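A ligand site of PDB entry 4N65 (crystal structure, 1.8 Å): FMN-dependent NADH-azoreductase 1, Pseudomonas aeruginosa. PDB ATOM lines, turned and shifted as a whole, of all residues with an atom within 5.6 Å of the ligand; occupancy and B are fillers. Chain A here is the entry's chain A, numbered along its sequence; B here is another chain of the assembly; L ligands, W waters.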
ATOM      1  N   SER A  10     -27.457 -16.314 -35.424  1.00  0.00           N
ATOM      2  CA  SER A  10     -27.415 -17.775 -35.364  1.00  0.00           C
ATOM      3  C   SER A  10     -27.749 -18.386 -36.734  1.00  0.00           C
ATOM      4  O   SER A  10     -28.692 -17.975 -37.396  1.00  0.00           O
ATOM      5  CB  SER A  10     -28.403 -18.333 -34.325  1.00  0.00           C
ATOM      6  OG  SER A  10     -28.399 -19.750 -34.469  1.00  0.00           O
ATOM      7  N   PRO A  11     -26.994 -19.412 -37.154  1.00  0.00           N
ATOM      8  CA  PRO A  11     -27.436 -20.159 -38.341  1.00  0.00           C
ATOM      9  C   PRO A  11     -28.669 -21.006 -38.125  1.00  0.00           C
ATOM     10  O   PRO A  11     -29.247 -21.461 -39.103  1.00  0.00           O
ATOM     11  CB  PRO A  11     -26.232 -21.039 -38.715  1.00  0.00           C
ATOM     12  CG  PRO A  11     -25.358 -21.047 -37.517  1.00  0.00           C
ATOM     13  CD  PRO A  11     -25.749 -19.945 -36.569  1.00  0.00           C
ATOM     14  N   ARG A  12     -29.108 -21.192 -36.879  1.00  0.00           N
ATOM     15  CA  ARG A  12     -30.305 -21.955 -36.617  1.00  0.00           C
ATOM     16  C   ARG A  12     -31.556 -21.112 -36.797  1.00  0.00           C
ATOM     17  O   ARG A  12     -31.527 -19.879 -36.669  1.00  0.00           O
ATOM     18  CB  ARG A  12     -30.257 -22.584 -35.220  1.00  0.00           C
ATOM     19  CG  ARG A  12     -28.976 -23.390 -35.011  1.00  0.00           C
ATOM     20  CD  ARG A  12     -29.109 -24.459 -33.956  1.00  0.00           C
ATOM     21  NE  ARG A  12     -29.332 -23.915 -32.622  1.00  0.00           N
ATOM     22  CZ  ARG A  12     -29.662 -24.655 -31.580  1.00  0.00           C
ATOM     23  NH1 ARG A  12     -29.820 -24.086 -30.402  1.00  0.00           N
ATOM     24  NH2 ARG A  12     -29.798 -25.998 -31.698  1.00  0.00           N
ATOM     25  N   ARG A  15     -35.051 -23.394 -33.982  1.00  0.00           N
ATOM     26  CA  ARG A  15     -34.335 -23.886 -32.797  1.00  0.00           C
ATOM     27  C   ARG A  15     -33.327 -22.900 -32.157  1.00  0.00           C
ATOM     28  O   ARG A  15     -32.786 -23.175 -31.063  1.00  0.00           O
ATOM     29  CB  ARG A  15     -33.635 -25.204 -33.128  1.00  0.00           C
ATOM     30  CG  ARG A  15     -34.604 -26.332 -33.363  1.00  0.00           C
ATOM     31  CD  ARG A  15     -33.905 -27.633 -33.578  1.00  0.00           C
ATOM     32  NE  ARG A  15     -34.902 -28.671 -33.807  1.00  0.00           N
ATOM     33  CZ  ARG A  15     -35.575 -29.311 -32.853  1.00  0.00           C
ATOM     34  NH1 ARG A  15     -35.322 -29.051 -31.580  1.00  0.00           N
ATOM     35  NH2 ARG A  15     -36.481 -30.215 -33.171  1.00  0.00           N
ATOM     36  N   SER A  16     -33.045 -21.789 -32.815  1.00  0.00           N
ATOM     37  CA  SER A  16     -32.129 -20.775 -32.236  1.00  0.00           C
ATOM     38  C   SER A  16     -32.749 -20.122 -31.020  1.00  0.00           C
ATOM     39  O   SER A  16     -33.826 -19.504 -31.116  1.00  0.00           O
ATOM     40  CB  SER A  16     -31.799 -19.645 -33.227  1.00  0.00           C
ATOM     41  OG  SER A  16     -31.098 -18.604 -32.553  1.00  0.00           O
ATOM     42  N   GLN A  17     -32.073 -20.248 -29.894  1.00  0.00           N
ATOM     43  CA  GLN A  17     -32.545 -19.583 -28.703  1.00  0.00           C
ATOM     44  C   GLN A  17     -32.235 -18.094 -28.717  1.00  0.00           C
ATOM     45  O   GLN A  17     -33.022 -17.319 -28.236  1.00  0.00           O
ATOM     46  CB  GLN A  17     -31.941 -20.240 -27.449  1.00  0.00           C
ATOM     47  CG  GLN A  17     -32.361 -21.675 -27.305  1.00  0.00           C
ATOM     48  CD  GLN A  17     -33.821 -21.845 -26.882  1.00  0.00           C
ATOM     49  OE1 GLN A  17     -34.516 -20.879 -26.536  1.00  0.00           O
ATOM     50  NE2 GLN A  17     -34.282 -23.095 -26.875  1.00  0.00           N
ATOM     51  N   SER A  18     -31.084 -17.688 -29.286  1.00  0.00           N
ATOM     52  CA  SER A  18     -30.814 -16.263 -29.338  1.00  0.00           C
ATOM     53  C   SER A  18     -31.839 -15.528 -30.246  1.00  0.00           C
ATOM     54  O   SER A  18     -32.312 -14.449 -29.896  1.00  0.00           O
ATOM     55  CB  SER A  18     -29.370 -15.963 -29.763  1.00  0.00           C
ATOM     56  OG  SER A  18     -29.048 -16.468 -31.060  1.00  0.00           O
ATOM     57  N   ARG A  19     -32.146 -16.127 -31.401  1.00  0.00           N
ATOM     58  CA  ARG A  19     -33.152 -15.600 -32.323  1.00  0.00           C
ATOM     59  C   ARG A  19     -34.505 -15.542 -31.640  1.00  0.00           C
ATOM     60  O   ARG A  19     -35.215 -14.538 -31.686  1.00  0.00           O
ATOM     61  CB  ARG A  19     -33.217 -16.487 -33.585  1.00  0.00           C
ATOM     62  CG  ARG A  19     -34.161 -16.008 -34.666  1.00  0.00           C
ATOM     63  CD  ARG A  19     -34.328 -17.071 -35.777  1.00  0.00           C
ATOM     64  NE  ARG A  19     -33.053 -17.374 -36.428  1.00  0.00           N
ATOM     65  CZ  ARG A  19     -32.519 -16.606 -37.379  1.00  0.00           C
ATOM     66  NH1 ARG A  19     -33.144 -15.489 -37.759  1.00  0.00           N
ATOM     67  NH2 ARG A  19     -31.370 -16.940 -37.933  1.00  0.00           N
ATOM     68  N   THR A  95     -27.089 -13.367 -31.083  1.00  0.00           N
ATOM     69  CA  THR A  95     -25.940 -14.203 -31.415  1.00  0.00           C
ATOM     70  C   THR A  95     -25.681 -15.330 -30.431  1.00  0.00           C
ATOM     71  O   THR A  95     -25.712 -15.139 -29.221  1.00  0.00           O
ATOM     72  CB  THR A  95     -24.653 -13.347 -31.574  1.00  0.00           C
ATOM     73  OG1 THR A  95     -23.602 -14.172 -32.063  1.00  0.00           O
ATOM     74  CG2 THR A  95     -24.208 -12.669 -30.277  1.00  0.00           C
ATOM     75  N   PRO A  96     -25.399 -16.520 -30.951  1.00  0.00           N
ATOM     76  CA  PRO A  96     -24.755 -17.534 -30.132  1.00  0.00           C
ATOM     77  C   PRO A  96     -23.354 -17.124 -29.715  1.00  0.00           C
ATOM     78  O   PRO A  96     -22.735 -16.269 -30.380  1.00  0.00           O
ATOM     79  CB  PRO A  96     -24.569 -18.703 -31.099  1.00  0.00           C
ATOM     80  CG  PRO A  96     -25.456 -18.439 -32.266  1.00  0.00           C
ATOM     81  CD  PRO A  96     -25.573 -16.956 -32.350  1.00  0.00           C
ATOM     82  N   MET A  97     -22.804 -17.828 -28.742  1.00  0.00           N
ATOM     83  CA  MET A  97     -21.361 -17.903 -28.602  1.00  0.00           C
ATOM     84  C   MET A  97     -20.881 -19.114 -29.376  1.00  0.00           C
ATOM     85  O   MET A  97     -21.272 -20.236 -29.084  1.00  0.00           O
ATOM     86  CB  MET A  97     -20.938 -18.023 -27.136  1.00  0.00           C
ATOM     87  CG  MET A  97     -19.436 -18.250 -26.977  1.00  0.00           C
ATOM     88  SD  MET A  97     -18.871 -18.286 -25.254  1.00  0.00           S
ATOM     89  CE  MET A  97     -18.871 -16.543 -24.851  1.00  0.00           C
ATOM     90  N   TYR A  98     -19.995 -18.880 -30.337  1.00  0.00           N
ATOM     91  CA  TYR A  98     -19.357 -19.963 -31.074  1.00  0.00           C
ATOM     92  C   TYR A  98     -17.850 -19.890 -30.846  1.00  0.00           C
ATOM     93  O   TYR A  98     -17.229 -18.902 -31.229  1.00  0.00           O
ATOM     94  CB  TYR A  98     -19.585 -19.794 -32.579  1.00  0.00           C
ATOM     95  CG  TYR A  98     -20.865 -20.405 -33.136  1.00  0.00           C
ATOM     96  CD1 TYR A  98     -21.857 -20.907 -32.310  1.00  0.00           C
ATOM     97  CD2 TYR A  98     -21.067 -20.478 -34.508  1.00  0.00           C
ATOM     98  CE1 TYR A  98     -23.025 -21.463 -32.839  1.00  0.00           C
ATOM     99  CE2 TYR A  98     -22.223 -21.042 -35.046  1.00  0.00           C
ATOM    100  CZ  TYR A  98     -23.193 -21.529 -34.196  1.00  0.00           C
ATOM    101  OH  TYR A  98     -24.321 -22.109 -34.737  1.00  0.00           O
ATOM    102  N   ASN A  99     -17.299 -20.934 -30.217  1.00  0.00           N
ATOM    103  CA  ASN A  99     -15.867 -21.017 -29.942  1.00  0.00           C
ATOM    104  C   ASN A  99     -15.309 -19.716 -29.325  1.00  0.00           C
ATOM    105  O   ASN A  99     -14.332 -19.140 -29.782  1.00  0.00           O
ATOM    106  CB  ASN A  99     -15.166 -21.473 -31.230  1.00  0.00           C
ATOM    107  CG  ASN A  99     -15.657 -22.859 -31.647  1.00  0.00           C
ATOM    108  OD1 ASN A  99     -15.711 -23.766 -30.821  1.00  0.00           O
ATOM    109  ND2 ASN A  99     -16.084 -23.009 -32.882  1.00  0.00           N
ATOM    110  N   PHE A 100     -15.978 -19.298 -28.253  1.00  0.00           N
ATOM    111  CA  PHE A 100     -15.591 -18.136 -27.445  1.00  0.00           C
ATOM    112  C   PHE A 100     -15.761 -16.783 -28.128  1.00  0.00           C
ATOM    113  O   PHE A 100     -15.417 -15.765 -27.541  1.00  0.00           O
ATOM    114  CB  PHE A 100     -14.175 -18.323 -26.904  1.00  0.00           C
ATOM    115  CG  PHE A 100     -13.985 -19.653 -26.275  1.00  0.00           C
ATOM    116  CD1 PHE A 100     -14.590 -19.956 -25.063  1.00  0.00           C
ATOM    117  CD2 PHE A 100     -13.275 -20.654 -26.940  1.00  0.00           C
ATOM    118  CE1 PHE A 100     -14.455 -21.206 -24.492  1.00  0.00           C
ATOM    119  CE2 PHE A 100     -13.119 -21.897 -26.352  1.00  0.00           C
ATOM    120  CZ  PHE A 100     -13.723 -22.175 -25.139  1.00  0.00           C
ATOM    121  N   SER A 101     -16.347 -16.773 -29.327  1.00  0.00           N
ATOM    122  CA  SER A 101     -16.607 -15.534 -30.017  1.00  0.00           C
ATOM    123  C   SER A 101     -17.986 -15.634 -30.659  1.00  0.00           C
ATOM    124  O   SER A 101     -18.883 -16.308 -30.108  1.00  0.00           O
ATOM    125  CB  SER A 101     -15.485 -15.300 -31.031  1.00  0.00           C
ATOM    126  OG  SER A 101     -15.598 -14.059 -31.698  1.00  0.00           O
ATOM    127  N   SER A 145     -26.909 -16.398 -26.439  1.00  0.00           N
ATOM    128  CA  SER A 145     -27.099 -17.707 -25.846  1.00  0.00           C
ATOM    129  C   SER A 145     -25.772 -18.473 -25.879  1.00  0.00           C
ATOM    130  O   SER A 145     -25.010 -18.365 -26.837  1.00  0.00           O
ATOM    131  CB  SER A 145     -28.167 -18.488 -26.611  1.00  0.00           C
ATOM    132  OG  SER A 145     -28.473 -19.687 -25.913  1.00  0.00           O
ATOM    133  N   ARG A 146     -25.502 -19.203 -24.805  1.00  0.00           N
ATOM    134  CA  ARG A 146     -24.250 -19.918 -24.644  1.00  0.00           C
ATOM    135  C   ARG A 146     -24.565 -21.323 -24.126  1.00  0.00           C
ATOM    136  O   ARG A 146     -25.472 -21.523 -23.308  1.00  0.00           O
ATOM    137  CB  ARG A 146     -23.359 -19.252 -23.583  1.00  0.00           C
ATOM    138  CG  ARG A 146     -23.210 -17.732 -23.745  1.00  0.00           C
ATOM    139  CD  ARG A 146     -22.165 -17.120 -22.811  1.00  0.00           C
ATOM    140  NE  ARG A 146     -22.241 -15.657 -22.933  1.00  0.00           N
ATOM    141  CZ  ARG A 146     -22.526 -14.814 -21.954  1.00  0.00           C
ATOM    142  NH1 ARG A 146     -22.733 -15.236 -20.696  1.00  0.00           N
ATOM    143  NH2 ARG A 146     -22.612 -13.521 -22.236  1.00  0.00           N
ATOM    144  N   GLY A 147     -23.798 -22.297 -24.602  1.00  0.00           N
ATOM    145  CA  GLY A 147     -24.003 -23.679 -24.183  1.00  0.00           C
ATOM    146  C   GLY A 147     -23.556 -23.883 -22.762  1.00  0.00           C
ATOM    147  O   GLY A 147     -24.199 -24.615 -22.001  1.00  0.00           O
ATOM    148  N   GLY A 148     -22.459 -23.214 -22.420  1.00  0.00           N
ATOM    149  CA  GLY A 148     -21.831 -23.399 -21.131  1.00  0.00           C
ATOM    150  C   GLY A 148     -22.251 -22.339 -20.134  1.00  0.00           C
ATOM    151  O   GLY A 148     -23.251 -21.657 -20.341  1.00  0.00           O
ATOM    152  N   HIS A 149     -21.499 -22.253 -19.047  1.00  0.00           N
ATOM    153  CA  HIS A 149     -21.801 -21.387 -17.906  1.00  0.00           C
ATOM    154  C   HIS A 149     -20.566 -20.573 -17.544  1.00  0.00           C
ATOM    155  O   HIS A 149     -19.446 -20.946 -17.899  1.00  0.00           O
ATOM    156  CB  HIS A 149     -22.164 -22.211 -16.652  1.00  0.00           C
ATOM    157  CG  HIS A 149     -23.498 -22.875 -16.725  1.00  0.00           C
ATOM    158  ND1 HIS A 149     -23.645 -24.246 -16.853  1.00  0.00           N
ATOM    159  CD2 HIS A 149     -24.757 -22.372 -16.662  1.00  0.00           C
ATOM    160  CE1 HIS A 149     -24.934 -24.545 -16.871  1.00  0.00           C
ATOM    161  NE2 HIS A 149     -25.626 -23.432 -16.762  1.00  0.00           N
ATOM    162  N   PHE A 151     -19.619 -17.401 -18.312  1.00  0.00           N
ATOM    163  CA  PHE A 151     -18.984 -16.487 -19.269  1.00  0.00           C
ATOM    164  C   PHE A 151     -19.296 -15.015 -18.970  1.00  0.00           C
ATOM    165  O   PHE A 151     -18.766 -14.107 -19.613  1.00  0.00           O
ATOM    166  CB  PHE A 151     -19.369 -16.834 -20.710  1.00  0.00           C
ATOM    167  CG  PHE A 151     -18.713 -18.097 -21.188  1.00  0.00           C
ATOM    168  CD1 PHE A 151     -17.375 -18.096 -21.552  1.00  0.00           C
ATOM    169  CD2 PHE A 151     -19.405 -19.282 -21.237  1.00  0.00           C
ATOM    170  CE1 PHE A 151     -16.745 -19.272 -21.970  1.00  0.00           C
ATOM    171  CE2 PHE A 151     -18.770 -20.454 -21.663  1.00  0.00           C
ATOM    172  CZ  PHE A 151     -17.450 -20.433 -22.014  1.00  0.00           C
ATOM    173  N   GLU A 187     -27.312 -23.857 -22.340  1.00  0.00           N
ATOM    174  CA  GLU A 187     -28.107 -24.420 -23.450  1.00  0.00           C
ATOM    175  C   GLU A 187     -27.784 -25.853 -23.787  1.00  0.00           C
ATOM    176  O   GLU A 187     -28.624 -26.570 -24.328  1.00  0.00           O
ATOM    177  CB  GLU A 187     -27.982 -23.572 -24.734  1.00  0.00           C
ATOM    178  CG  GLU A 187     -29.070 -23.865 -25.783  1.00  0.00           C
ATOM    179  CD  GLU A 187     -28.728 -24.982 -26.746  1.00  0.00           C
ATOM    180  OE1 GLU A 187     -27.585 -25.488 -26.702  1.00  0.00           O
ATOM    181  OE2 GLU A 187     -29.610 -25.359 -27.552  1.00  0.00           O
ATOM    182  N   GLU A 188     -26.575 -26.271 -23.470  1.00  0.00           N
ATOM    183  CA  GLU A 188     -26.143 -27.606 -23.835  1.00  0.00           C
ATOM    184  C   GLU A 188     -26.690 -28.637 -22.830  1.00  0.00           C
ATOM    185  O   GLU A 188     -27.180 -29.694 -23.218  1.00  0.00           O
ATOM    186  CB  GLU A 188     -24.625 -27.656 -23.941  1.00  0.00           C
ATOM    187  CG  GLU A 188     -24.125 -28.278 -25.234  1.00  0.00           C
ATOM    188  CD  GLU A 188     -23.265 -27.353 -26.083  1.00  0.00           C
ATOM    189  OE1 GLU A 188     -22.355 -26.673 -25.528  1.00  0.00           O
ATOM    190  OE2 GLU A 188     -23.484 -27.325 -27.313  1.00  0.00           O
ATOM    191  N   PHE A 194     -31.348 -24.291 -17.643  1.00  0.00           N
ATOM    192  CA  PHE A 194     -31.447 -23.524 -18.887  1.00  0.00           C
ATOM    193  C   PHE A 194     -32.848 -22.923 -19.001  1.00  0.00           C
ATOM    194  O   PHE A 194     -33.024 -21.822 -19.510  1.00  0.00           O
ATOM    195  CB  PHE A 194     -31.180 -24.424 -20.073  1.00  0.00           C
ATOM    196  CG  PHE A 194     -31.320 -23.736 -21.404  1.00  0.00           C
ATOM    197  CD1 PHE A 194     -30.347 -22.855 -21.849  1.00  0.00           C
ATOM    198  CD2 PHE A 194     -32.427 -23.960 -22.198  1.00  0.00           C
ATOM    199  CE1 PHE A 194     -30.477 -22.223 -23.071  1.00  0.00           C
ATOM    200  CE2 PHE A 194     -32.570 -23.328 -23.416  1.00  0.00           C
ATOM    201  CZ  PHE A 194     -31.582 -22.464 -23.859  1.00  0.00           C
ATOM    202  N   VAL B  51     -20.245 -21.986 -40.464  1.00  0.00           N
ATOM    203  CA  VAL B  51     -21.078 -23.041 -39.875  1.00  0.00           C
ATOM    204  C   VAL B  51     -22.532 -22.785 -40.173  1.00  0.00           C
ATOM    205  O   VAL B  51     -23.028 -21.676 -39.996  1.00  0.00           O
ATOM    206  CB  VAL B  51     -20.832 -23.096 -38.359  1.00  0.00           C
ATOM    207  CG1 VAL B  51     -21.982 -23.816 -37.567  1.00  0.00           C
ATOM    208  CG2 VAL B  51     -19.535 -23.797 -38.145  1.00  0.00           C
ATOM    209  N   PHE B  55     -24.321 -28.165 -40.558  1.00  0.00           N
ATOM    210  CA  PHE B  55     -23.069 -28.474 -39.851  1.00  0.00           C
ATOM    211  C   PHE B  55     -23.317 -28.833 -38.410  1.00  0.00           C
ATOM    212  O   PHE B  55     -22.834 -29.845 -37.959  1.00  0.00           O
ATOM    213  CB  PHE B  55     -22.128 -27.280 -39.907  1.00  0.00           C
ATOM    214  CG  PHE B  55     -20.825 -27.472 -39.151  1.00  0.00           C
ATOM    215  CD1 PHE B  55     -20.738 -27.238 -37.794  1.00  0.00           C
ATOM    216  CD2 PHE B  55     -19.661 -27.823 -39.825  1.00  0.00           C
ATOM    217  CE1 PHE B  55     -19.539 -27.366 -37.114  1.00  0.00           C
ATOM    218  CE2 PHE B  55     -18.460 -27.943 -39.139  1.00  0.00           C
ATOM    219  CZ  PHE B  55     -18.411 -27.720 -37.789  1.00  0.00           C
ATOM    220  N   VAL B  56     -24.087 -28.005 -37.697  1.00  0.00           N
ATOM    221  CA  VAL B  56     -24.362 -28.256 -36.292  1.00  0.00           C
ATOM    222  C   VAL B  56     -25.036 -29.605 -36.087  1.00  0.00           C
ATOM    223  O   VAL B  56     -24.614 -30.366 -35.222  1.00  0.00           O
ATOM    224  CB  VAL B  56     -25.201 -27.143 -35.639  1.00  0.00           C
ATOM    225  CG1 VAL B  56     -25.510 -27.490 -34.179  1.00  0.00           C
ATOM    226  CG2 VAL B  56     -24.492 -25.789 -35.776  1.00  0.00           C
ATOM    227  N   PHE B  60     -22.683 -32.368 -34.053  1.00  0.00           N
ATOM    228  CA  PHE B  60     -23.137 -32.713 -32.706  1.00  0.00           C
ATOM    229  C   PHE B  60     -24.035 -33.919 -32.682  1.00  0.00           C
ATOM    230  O   PHE B  60     -24.682 -34.198 -31.661  1.00  0.00           O
ATOM    231  CB  PHE B  60     -23.773 -31.498 -32.013  1.00  0.00           C
ATOM    232  CG  PHE B  60     -22.799 -30.432 -31.661  1.00  0.00           C
ATOM    233  CD1 PHE B  60     -22.380 -29.508 -32.602  1.00  0.00           C
ATOM    234  CD2 PHE B  60     -22.244 -30.382 -30.396  1.00  0.00           C
ATOM    235  CE1 PHE B  60     -21.446 -28.527 -32.259  1.00  0.00           C
ATOM    236  CE2 PHE B  60     -21.303 -29.414 -30.056  1.00  0.00           C
ATOM    237  CZ  PHE B  60     -20.914 -28.503 -30.970  1.00  0.00           C
ATOM    238  N   ASP B 111     -14.210 -22.232 -36.565  1.00  0.00           N
ATOM    239  CA  ASP B 111     -15.529 -22.850 -36.412  1.00  0.00           C
ATOM    240  C   ASP B 111     -15.622 -24.205 -37.128  1.00  0.00           C
ATOM    241  O   ASP B 111     -16.415 -25.041 -36.747  1.00  0.00           O
ATOM    242  CB  ASP B 111     -16.670 -21.918 -36.868  1.00  0.00           C
ATOM    243  CG  ASP B 111     -16.881 -20.736 -35.911  1.00  0.00           C
ATOM    244  OD1 ASP B 111     -16.335 -20.804 -34.774  1.00  0.00           O
ATOM    245  OD2 ASP B 111     -17.557 -19.744 -36.293  1.00  0.00           O
HETATM  246  N1  LIG L   1     -21.162 -22.621 -26.058  1.00  0.00           N
HETATM  247  C1  LIG L   1     -20.313 -22.031 -25.138  1.00  0.00           C
HETATM  248  O1  LIG L   1     -20.697 -21.844 -23.974  1.00  0.00           O
HETATM  249  N2  LIG L   1     -19.071 -21.653 -25.525  1.00  0.00           N
HETATM  250  C2  LIG L   1     -18.638 -21.845 -26.819  1.00  0.00           C
HETATM  251  O2  LIG L   1     -17.496 -21.451 -27.145  1.00  0.00           O
HETATM  252  C3  LIG L   1     -19.506 -22.463 -27.728  1.00  0.00           C
HETATM  253  N3  LIG L   1     -19.149 -22.700 -29.007  1.00  0.00           N
HETATM  254  C4  LIG L   1     -20.020 -23.285 -29.927  1.00  0.00           C
HETATM  255  C5  LIG L   1     -19.602 -23.485 -31.222  1.00  0.00           C
HETATM  256  C6  LIG L   1     -20.463 -24.067 -32.133  1.00  0.00           C
HETATM  257  C7  LIG L   1     -19.987 -24.226 -33.553  1.00  0.00           C
HETATM  258  C8  LIG L   1     -21.753 -24.458 -31.732  1.00  0.00           C
HETATM  259  C9  LIG L   1     -22.757 -25.070 -32.679  1.00  0.00           C
HETATM  260  C10 LIG L   1     -22.155 -24.250 -30.435  1.00  0.00           C
HETATM  261  C11 LIG L   1     -21.284 -23.664 -29.515  1.00  0.00           C
HETATM  262  N4  LIG L   1     -21.648 -23.445 -28.211  1.00  0.00           N
HETATM  263  C12 LIG L   1     -20.773 -22.834 -27.328  1.00  0.00           C
HETATM  264  C13 LIG L   1     -23.015 -23.756 -27.724  1.00  0.00           C
HETATM  265  C14 LIG L   1     -23.877 -22.552 -28.206  1.00  0.00           C
HETATM  266  O3  LIG L   1     -23.390 -21.289 -27.755  1.00  0.00           O
HETATM  267  C15 LIG L   1     -25.328 -22.657 -27.753  1.00  0.00           C
HETATM  268  O4  LIG L   1     -25.837 -23.865 -28.255  1.00  0.00           O
HETATM  269  C16 LIG L   1     -26.237 -21.508 -28.246  1.00  0.00           C
HETATM  270  O5  LIG L   1     -27.451 -21.588 -27.519  1.00  0.00           O
HETATM  271  C17 LIG L   1     -26.517 -21.515 -29.755  1.00  0.00           C
HETATM  272  O6  LIG L   1     -27.230 -20.341 -30.083  1.00  0.00           O
HETATM  273  P1  LIG L   1     -28.615 -20.503 -30.845  1.00  0.00           P
HETATM  274  O7  LIG L   1     -29.478 -21.355 -29.956  1.00  0.00           O
HETATM  275  O8  LIG L   1     -28.340 -21.174 -32.176  1.00  0.00           O
HETATM  276  O9  LIG L   1     -29.212 -19.131 -31.032  1.00  0.00           O
HETATM  277  O   HOH W   1     -26.176 -22.821 -32.920  1.00  0.00           O
HETATM  278  O   HOH W   2     -17.007 -25.522 -34.159  1.00  0.00           O
HETATM  279  O   HOH W   3     -18.356 -27.191 -32.679  1.00  0.00           O
HETATM  280  O   HOH W   4     -25.949 -24.910 -30.937  1.00  0.00           O
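The backbone NH (N) of Gly 148 sits at hydrogen-bond distance from an oxygen (O1) of the ligand (2.7 Å).
O3 of the ligand is in hydrogen-bond range of O of Ser 145.
OG of Ser 145 is in hydrogen-bond range of O5 of the ligand (2.7 Å).
The backbone NH (N) of Gly 147 is in hydrogen-bond range of a nitrogen (N1) of the ligand (3.0 Å).
The backbone NH of Asn 99 is in hydrogen-bond range of a nitrogen (N3) of the ligand.
OG of Ser 18 sits at hydrogen-bond distance from O9 of the ligand (2.7 Å).
The side-chain carboxylate of Glu 187 is in hydrogen-bond range of an oxygen (O4) of the ligand, 2.8 Å away.
OG of Ser 16 sits at hydrogen-bond distance from O9 of the ligand, at 2.5 Å.
O of Met 97 is in hydrogen-bond range of O3 of the ligand, at 2.7 Å.
O8 of the ligand sits at hydrogen-bond distance from OG of Ser 10.
The backbone NH (N) of Phe 100 sits at hydrogen-bond distance from an oxygen (O2) of the ligand, 2.9 Å away.
N of Ser 18 lies within hydrogen-bond range of O9 of the ligand (2.9 Å).
An oxygen (O7) of the ligand lies within hydrogen-bond range of the backbone NH (N) of Gln 17.
The guanidinium group (NH1) of Arg 12 lies within salt-bridge range of an oxygen (O7) of the ligand.
A nitrogen (N2) of the ligand lies within hydrogen-bond range of the side-chain sulfur (SD) of Met 97, 3.4 Å away.
The backbone carbonyl oxygen (O) of Ser 10 lies within hydrogen-bond range of the guanidinium group (NH2) of Arg 19 (2.9 Å).
The backbone NH (N) of Glu 187 lies within hydrogen-bond range of the backbone carbonyl oxygen (O) of Arg 146 (3.1 Å).
The backbone carbonyl oxygen (O) of Ser 145 is in hydrogen-bond range of the backbone NH (N) of Met 97, 3.0 Å away.
The guanidinium group of Arg 12 is in salt-bridge range of the side-chain carboxylate of Glu 187.
ND2 of Asn 99 lies within hydrogen-bond range of OD1 of Asp 111 of chain B, 2.9 Å away.
OG of Ser 10 lies within hydrogen-bond range of N of Arg 12 (2.9 Å).
N of Glu 187 sits at hydrogen-bond distance from O of Gly 147.
N of Ser 145 lies within hydrogen-bond range of O of Thr 95 (3.3 Å).
Merely in contact with the ligand: Pro 96 (3.3 Å), Phe 151 (3.3 Å), Tyr 98 (3.4 Å), Arg 146 (3.5 Å), Val 56 of chain B (3.6 Å), Glu 188 (3.6 Å), Phe 60 of chain B (3.7 Å) and Arg 15 (3.9 Å).
Within 4 Å of the ligand: Ser 10, Arg 12, Arg 15, Ser 16, Gln 17, Ser 18, Pro 96, Met 97, Tyr 98, Asn 99, Phe 100, Ser 145, Arg 146, Gly 147, Gly 148, Phe 151, Glu 187, Glu 188, Val 56 of chain B and Phe 60 of chain B.
Water W1 lies within hydrogen-bond range of OH of Tyr 98 (2.7 Å), O8 of the ligand (2.8 Å) and NE of Arg 12 (3.4 Å).
Water W2 lies within hydrogen-bond range of O of Asp 111 of chain B (2.7 Å) and ND2 of Asn 99 (3.0 Å).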
